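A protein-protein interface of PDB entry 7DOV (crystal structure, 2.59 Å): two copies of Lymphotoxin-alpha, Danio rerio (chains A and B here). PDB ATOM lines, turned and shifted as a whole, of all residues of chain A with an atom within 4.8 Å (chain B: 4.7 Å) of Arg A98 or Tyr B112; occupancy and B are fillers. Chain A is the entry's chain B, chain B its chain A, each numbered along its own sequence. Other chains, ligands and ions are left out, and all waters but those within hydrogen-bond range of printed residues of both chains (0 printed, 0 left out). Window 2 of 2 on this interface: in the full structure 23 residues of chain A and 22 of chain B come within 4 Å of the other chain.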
ATOM      1  N   GLN A  73       7.660 -27.770  21.974  1.00  0.00           N
ATOM      2  CA  GLN A  73       7.284 -26.722  20.989  1.00  0.00           C
ATOM      3  C   GLN A  73       8.414 -26.351  20.026  1.00  0.00           C
ATOM      4  O   GLN A  73       9.303 -25.612  20.441  1.00  0.00           O
ATOM      5  CB  GLN A  73       6.907 -25.477  21.785  1.00  0.00           C
ATOM      6  CG  GLN A  73       6.584 -24.269  20.933  1.00  0.00           C
ATOM      7  CD  GLN A  73       5.234 -23.717  21.303  1.00  0.00           C
ATOM      8  OE1 GLN A  73       4.390 -24.418  21.860  1.00  0.00           O
ATOM      9  NE2 GLN A  73       5.020 -22.452  20.989  1.00  0.00           N
ATOM     10  N   LEU A  75       9.446 -24.373  16.389  1.00  0.00           N
ATOM     11  CA  LEU A  75       8.766 -23.364  15.547  1.00  0.00           C
ATOM     12  C   LEU A  75       9.396 -23.284  14.163  1.00  0.00           C
ATOM     13  O   LEU A  75      10.547 -23.596  14.046  1.00  0.00           O
ATOM     14  CB  LEU A  75       8.904 -22.004  16.222  1.00  0.00           C
ATOM     15  CG  LEU A  75       8.389 -21.922  17.649  1.00  0.00           C
ATOM     16  CD1 LEU A  75       8.988 -20.716  18.342  1.00  0.00           C
ATOM     17  CD2 LEU A  75       6.885 -21.838  17.662  1.00  0.00           C
ATOM     18  N   MET A  76       8.626 -22.855  13.179  1.00  0.00           N
ATOM     19  CA  MET A  76       9.214 -22.630  11.843  1.00  0.00           C
ATOM     20  C   MET A  76       9.842 -21.240  11.871  1.00  0.00           C
ATOM     21  O   MET A  76       9.126 -20.296  12.073  1.00  0.00           O
ATOM     22  CB  MET A  76       8.121 -22.659  10.782  1.00  0.00           C
ATOM     23  CG  MET A  76       8.625 -22.816   9.391  1.00  0.00           C
ATOM     24  SD  MET A  76       7.243 -23.003   8.290  1.00  0.00           S
ATOM     25  CE  MET A  76       8.090 -23.013   6.723  1.00  0.00           C
ATOM     26  N   ALA A  96      11.237 -14.542   9.876  1.00  0.00           N
ATOM     27  CA  ALA A  96       9.802 -14.826  10.036  1.00  0.00           C
ATOM     28  C   ALA A  96       9.682 -16.081  10.895  1.00  0.00           C
ATOM     29  O   ALA A  96      10.573 -16.893  10.869  1.00  0.00           O
ATOM     30  CB  ALA A  96       9.126 -14.951   8.705  1.00  0.00           C
ATOM     31  N   ILE A  97       8.586 -16.211  11.622  1.00  0.00           N
ATOM     32  CA  ILE A  97       8.451 -17.351  12.560  1.00  0.00           C
ATOM     33  C   ILE A  97       7.023 -17.863  12.521  1.00  0.00           C
ATOM     34  O   ILE A  97       6.128 -17.069  12.433  1.00  0.00           O
ATOM     35  CB  ILE A  97       8.804 -16.860  13.966  1.00  0.00           C
ATOM     36  CG1 ILE A  97       9.223 -18.006  14.870  1.00  0.00           C
ATOM     37  CG2 ILE A  97       7.653 -16.069  14.540  1.00  0.00           C
ATOM     38  CD1 ILE A  97      10.695 -18.115  14.991  1.00  0.00           C
ATOM     39  N   ARG A  98       6.840 -19.166  12.589  1.00  0.00           N
ATOM     40  CA  ARG A  98       5.456 -19.681  12.598  1.00  0.00           C
ATOM     41  C   ARG A  98       5.364 -20.872  13.542  1.00  0.00           C
ATOM     42  O   ARG A  98       6.364 -21.542  13.743  1.00  0.00           O
ATOM     43  CB  ARG A  98       5.033 -20.111  11.198  1.00  0.00           C
ATOM     44  CG  ARG A  98       4.584 -18.954  10.330  1.00  0.00           C
ATOM     45  CD  ARG A  98       3.998 -19.394   9.014  1.00  0.00           C
ATOM     46  NE  ARG A  98       3.939 -18.224   8.171  1.00  0.00           N
ATOM     47  CZ  ARG A  98       3.945 -18.267   6.857  1.00  0.00           C
ATOM     48  NH1 ARG A  98       4.016 -19.426   6.233  1.00  0.00           N
ATOM     49  NH2 ARG A  98       3.909 -17.152   6.163  1.00  0.00           N
ATOM     50  N   SER A  99       4.191 -21.063  14.125  1.00  0.00           N
ATOM     51  CA  SER A  99       3.909 -22.239  14.976  1.00  0.00           C
ATOM     52  C   SER A  99       3.602 -23.371  14.007  1.00  0.00           C
ATOM     53  O   SER A  99       2.762 -23.164  13.163  1.00  0.00           O
ATOM     54  CB  SER A  99       2.711 -21.970  15.843  1.00  0.00           C
ATOM     55  OG  SER A  99       3.036 -21.163  16.956  1.00  0.00           O
ATOM     56  N   ILE A 100       4.284 -24.506  14.115  1.00  0.00           N
ATOM     57  CA  ILE A 100       4.034 -25.653  13.192  1.00  0.00           C
ATOM     58  C   ILE A 100       3.117 -26.661  13.870  1.00  0.00           C
ATOM     59  O   ILE A 100       2.874 -26.515  15.062  1.00  0.00           O
ATOM     60  CB  ILE A 100       5.348 -26.343  12.801  1.00  0.00           C
ATOM     61  CG1 ILE A 100       6.166 -26.726  14.030  1.00  0.00           C
ATOM     62  CG2 ILE A 100       6.152 -25.498  11.841  1.00  0.00           C
ATOM     63  CD1 ILE A 100       7.280 -27.682  13.745  1.00  0.00           C
ATOM     64  N   ASN A 113       3.900 -26.193   4.977  1.00  0.00           N
ATOM     65  CA  ASN A 113       3.892 -24.744   5.225  1.00  0.00           C
ATOM     66  C   ASN A 113       5.109 -24.098   4.604  1.00  0.00           C
ATOM     67  O   ASN A 113       6.183 -24.574   4.760  1.00  0.00           O
ATOM     68  CB  ASN A 113       3.633 -24.334   6.667  1.00  0.00           C
ATOM     69  CG  ASN A 113       2.919 -23.011   6.653  1.00  0.00           C
ATOM     70  OD1 ASN A 113       2.918 -22.332   5.649  1.00  0.00           O
ATOM     71  ND2 ASN A 113       2.288 -22.652   7.739  1.00  0.00           N
ATOM     72  N   THR A 114       4.887 -22.967   3.962  1.00  0.00           N
ATOM     73  CA  THR A 114       5.923 -22.220   3.220  1.00  0.00           C
ATOM     74  C   THR A 114       6.221 -20.921   3.946  1.00  0.00           C
ATOM     75  O   THR A 114       5.361 -20.423   4.431  1.00  0.00           O
ATOM     76  CB  THR A 114       5.343 -21.868   1.852  1.00  0.00           C
ATOM     77  OG1 THR A 114       6.155 -22.513   0.893  1.00  0.00           O
ATOM     78  CG2 THR A 114       5.323 -20.396   1.529  1.00  0.00           C
ATOM     79  N   ILE A 115       7.444 -20.406   4.012  1.00  0.00           N
ATOM     80  CA  ILE A 115       7.660 -19.054   4.618  1.00  0.00           C
ATOM     81  C   ILE A 115       8.364 -18.149   3.604  1.00  0.00           C
ATOM     82  O   ILE A 115       9.405 -18.529   3.144  1.00  0.00           O
ATOM     83  CB  ILE A 115       8.469 -19.084   5.927  1.00  0.00           C
ATOM     84  CG1 ILE A 115       7.608 -19.430   7.135  1.00  0.00           C
ATOM     85  CG2 ILE A 115       9.162 -17.756   6.154  1.00  0.00           C
ATOM     86  CD1 ILE A 115       8.253 -19.111   8.445  1.00  0.00           C
ATOM     87  N   LEU B  61       3.752 -11.904  15.290  1.00  0.00           N
ATOM     88  CA  LEU B  61       3.045 -11.973  16.585  1.00  0.00           C
ATOM     89  C   LEU B  61       3.326 -13.291  17.295  1.00  0.00           C
ATOM     90  O   LEU B  61       3.485 -14.294  16.629  1.00  0.00           O
ATOM     91  CB  LEU B  61       1.541 -11.938  16.337  1.00  0.00           C
ATOM     92  CG  LEU B  61       0.963 -10.736  15.611  1.00  0.00           C
ATOM     93  CD1 LEU B  61      -0.514 -10.958  15.391  1.00  0.00           C
ATOM     94  CD2 LEU B  61       1.187  -9.453  16.376  1.00  0.00           C
ATOM     95  N   HIS B  62       3.382 -13.229  18.623  1.00  0.00           N
ATOM     96  CA  HIS B  62       3.347 -14.418  19.506  1.00  0.00           C
ATOM     97  C   HIS B  62       2.166 -14.162  20.425  1.00  0.00           C
ATOM     98  O   HIS B  62       2.177 -13.175  21.123  1.00  0.00           O
ATOM     99  CB  HIS B  62       4.613 -14.663  20.311  1.00  0.00           C
ATOM    100  CG  HIS B  62       4.991 -13.546  21.208  1.00  0.00           C
ATOM    101  ND1 HIS B  62       4.580 -12.255  20.990  1.00  0.00           N
ATOM    102  CD2 HIS B  62       5.897 -13.482  22.199  1.00  0.00           C
ATOM    103  CE1 HIS B  62       5.139 -11.454  21.869  1.00  0.00           C
ATOM    104  NE2 HIS B  62       5.943 -12.186  22.622  1.00  0.00           N
ATOM    105  N   ARG B  98      -5.513 -13.579   8.539  1.00  0.00           N
ATOM    106  CA  ARG B  98      -5.129 -14.970   8.853  1.00  0.00           C
ATOM    107  C   ARG B  98      -5.832 -15.450  10.123  1.00  0.00           C
ATOM    108  O   ARG B  98      -5.894 -14.688  11.083  1.00  0.00           O
ATOM    109  CB  ARG B  98      -3.610 -15.001   8.974  1.00  0.00           C
ATOM    110  CG  ARG B  98      -3.066 -16.247   9.633  1.00  0.00           C
ATOM    111  CD  ARG B  98      -2.148 -16.917   8.655  1.00  0.00           C
ATOM    112  NE  ARG B  98      -1.415 -15.952   7.865  1.00  0.00           N
ATOM    113  CZ  ARG B  98      -0.230 -16.227   7.369  1.00  0.00           C
ATOM    114  NH1 ARG B  98       0.291 -17.412   7.613  1.00  0.00           N
ATOM    115  NH2 ARG B  98       0.423 -15.346   6.644  1.00  0.00           N
ATOM    116  N   LEU B 110       2.369 -20.638  23.580  1.00  0.00           N
ATOM    117  CA  LEU B 110       2.145 -19.400  22.784  1.00  0.00           C
ATOM    118  C   LEU B 110       2.083 -19.746  21.287  1.00  0.00           C
ATOM    119  O   LEU B 110       2.868 -20.578  20.837  1.00  0.00           O
ATOM    120  CB  LEU B 110       3.339 -18.483  23.034  1.00  0.00           C
ATOM    121  CG  LEU B 110       3.049 -17.201  23.800  1.00  0.00           C
ATOM    122  CD1 LEU B 110       2.744 -17.515  25.238  1.00  0.00           C
ATOM    123  CD2 LEU B 110       4.220 -16.244  23.715  1.00  0.00           C
ATOM    124  N   TRP B 111       1.180 -19.075  20.568  1.00  0.00           N
ATOM    125  CA  TRP B 111       0.958 -19.235  19.108  1.00  0.00           C
ATOM    126  C   TRP B 111       1.676 -18.123  18.338  1.00  0.00           C
ATOM    127  O   TRP B 111       1.377 -16.947  18.569  1.00  0.00           O
ATOM    128  CB  TRP B 111      -0.535 -19.224  18.801  1.00  0.00           C
ATOM    129  CG  TRP B 111      -0.870 -19.635  17.403  1.00  0.00           C
ATOM    130  CD1 TRP B 111      -0.962 -20.902  16.922  1.00  0.00           C
ATOM    131  CD2 TRP B 111      -1.164 -18.769  16.299  1.00  0.00           C
ATOM    132  NE1 TRP B 111      -1.283 -20.884  15.597  1.00  0.00           N
ATOM    133  CE2 TRP B 111      -1.408 -19.590  15.188  1.00  0.00           C
ATOM    134  CE3 TRP B 111      -1.233 -17.386  16.140  1.00  0.00           C
ATOM    135  CZ2 TRP B 111      -1.731 -19.071  13.941  1.00  0.00           C
ATOM    136  CZ3 TRP B 111      -1.549 -16.873  14.908  1.00  0.00           C
ATOM    137  CH2 TRP B 111      -1.801 -17.707  13.827  1.00  0.00           C
ATOM    138  N   TYR B 112       2.547 -18.516  17.414  1.00  0.00           N
ATOM    139  CA  TYR B 112       3.371 -17.569  16.631  1.00  0.00           C
ATOM    140  C   TYR B 112       2.970 -17.528  15.157  1.00  0.00           C
ATOM    141  O   TYR B 112       2.879 -18.565  14.535  1.00  0.00           O
ATOM    142  CB  TYR B 112       4.809 -18.075  16.600  1.00  0.00           C
ATOM    143  CG  TYR B 112       5.606 -17.864  17.850  1.00  0.00           C
ATOM    144  CD1 TYR B 112       5.568 -18.771  18.888  1.00  0.00           C
ATOM    145  CD2 TYR B 112       6.426 -16.769  17.976  1.00  0.00           C
ATOM    146  CE1 TYR B 112       6.323 -18.586  20.030  1.00  0.00           C
ATOM    147  CE2 TYR B 112       7.187 -16.569  19.104  1.00  0.00           C
ATOM    148  CZ  TYR B 112       7.135 -17.478  20.133  1.00  0.00           C
ATOM    149  OH  TYR B 112       7.872 -17.246  21.246  1.00  0.00           O
ATOM    150  N   ASN B 113       2.787 -16.327  14.617  1.00  0.00           N
ATOM    151  CA  ASN B 113       2.538 -16.205  13.164  1.00  0.00           C
ATOM    152  C   ASN B 113       3.027 -14.876  12.606  1.00  0.00           C
ATOM    153  O   ASN B 113       3.284 -13.961  13.363  1.00  0.00           O
ATOM    154  CB  ASN B 113       1.132 -16.565  12.723  1.00  0.00           C
ATOM    155  CG  ASN B 113       1.189 -17.435  11.494  1.00  0.00           C
ATOM    156  OD1 ASN B 113       1.917 -17.145  10.570  1.00  0.00           O
ATOM    157  ND2 ASN B 113       0.476 -18.538  11.508  1.00  0.00           N
ATOM    158  N   THR B 114       3.164 -14.827  11.285  1.00  0.00           N
ATOM    159  CA  THR B 114       3.661 -13.638  10.564  1.00  0.00           C
ATOM    160  C   THR B 114       2.814 -13.397   9.325  1.00  0.00           C
ATOM    161  O   THR B 114       2.279 -14.338   8.787  1.00  0.00           O
ATOM    162  CB  THR B 114       5.074 -13.886  10.034  1.00  0.00           C
ATOM    163  OG1 THR B 114       5.823 -14.465  11.085  1.00  0.00           O
ATOM    164  CG2 THR B 114       5.804 -12.625   9.666  1.00  0.00           C
ATOM    165  N   GLU B 142       6.068  -8.680  17.772  1.00  0.00           N
ATOM    166  CA  GLU B 142       7.494  -8.848  18.140  1.00  0.00           C
ATOM    167  C   GLU B 142       8.276  -7.629  17.652  1.00  0.00           C
ATOM    168  O   GLU B 142       8.018  -7.182  16.563  1.00  0.00           O
ATOM    169  CB  GLU B 142       8.020 -10.106  17.481  1.00  0.00           C
ATOM    170  CG  GLU B 142       7.083 -11.270  17.674  1.00  0.00           C
ATOM    171  CD  GLU B 142       7.716 -12.470  18.349  1.00  0.00           C
ATOM    172  OE1 GLU B 142       8.416 -13.239  17.666  1.00  0.00           O
ATOM    173  OE2 GLU B 142       7.526 -12.612  19.551  1.00  0.00           O
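Arg A98 touches just these residues of chain B: Arg B98, Tyr B112 and Asn B113.
Tyr B112 touches just these residues of chain A: Leu A75, Ile A97, Arg A98 and Ser A99.
Of the printed residues of chain B, Ser A99 touches Leu B110, Trp B111 and Tyr B112.
Printed residues of chain A within 4 Å of Arg B98: Arg A98 (3.8 Å).
Of the printed residues of chain A, Thr B114 touches Ile A97.
Printed residues of chain B within 4 Å of Leu A75: Tyr B112 (3.6 Å).
Printed residues of chain B within 4 Å of Ile A97: Tyr B112, Asn B113 and Thr B114.
Thr A114 touches none of the printed residues of chain B.
Ile A100 touches none of the printed residues of chain B.
The nearest residue of chain A that does not touch Tyr B112 is Gln A73 (4.2 Å).
The nearest printed residue of chain B that does not touch Leu A75 is Leu B110 (5.3 Å).
N of Leu B61 sits at hydrogen-bond distance from O of Asn B113 (2.9 Å).
OD1 of Asn B113 lies within hydrogen-bond range of NH1 of Arg B98 (3.4 Å).
The guanidinium group of Arg B98 lies within hydrogen-bond range of the backbone carbonyl oxygen of Thr B114 (3.0 Å).
O of Met A76 lies within hydrogen-bond range of N of Arg A98, 2.6 Å away.
The side-chain amide oxygen (OD1) of Asn A113 is in hydrogen-bond range of the guanidinium group (NH1) of Arg A98 (3.2 Å).
NH1 of Arg A98 sits at hydrogen-bond distance from O of Thr A114 (2.5 Å).
The side-chain amide nitrogen (NE2) of Gln A73 lies within hydrogen-bond range of the backbone carbonyl oxygen (O) of Leu B110, 2.9 Å away.
The backbone NH of Tyr B112 is in hydrogen-bond range of the side-chain hydroxyl of Ser A99, at 2.7 Å.
The side-chain amide oxygen (OD1) of Asn B113 lies close to the guanidinium group (NE) of Arg A98 (3.3 Å).
O of Ile A97 is in hydrogen-bond range of OG1 of Thr B114 (2.9 Å).
Among the printed residues, pairs that only touch across the chains: Leu A75 with Tyr B112, Ile A97 with Tyr B112, Ile A97 with Asn B113, Arg A98 with Arg B98, Arg A98 with Tyr B112, Ser A99 with Leu B110 and Ser A99 with Trp B111.
Arg B98 touches its own counterpart, Arg A98.
Arg A98 touches Asn B113, but with the chains exchanged Asn A113 does not touch Arg B98 (5.6 Å).
Of the 11 pairs that touch across the chains among the printed residues, 1 has its exchanged pair printed and touching as well.
Of the 9 printed residues of chain B, 6 touch a printed residue of chain A.
Of the 11 printed residues of chain A, 5 touch a printed residue of chain B.
Hydrophobic or aromatic side chains of chain A within 4 Å of the printed part of chain B: Leu A75 and Ile A97.
Among the printed residues, no Asp or Glu carboxylate lies within 4 Å of a Lys or Arg side-chain nitrogen of the other chain.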
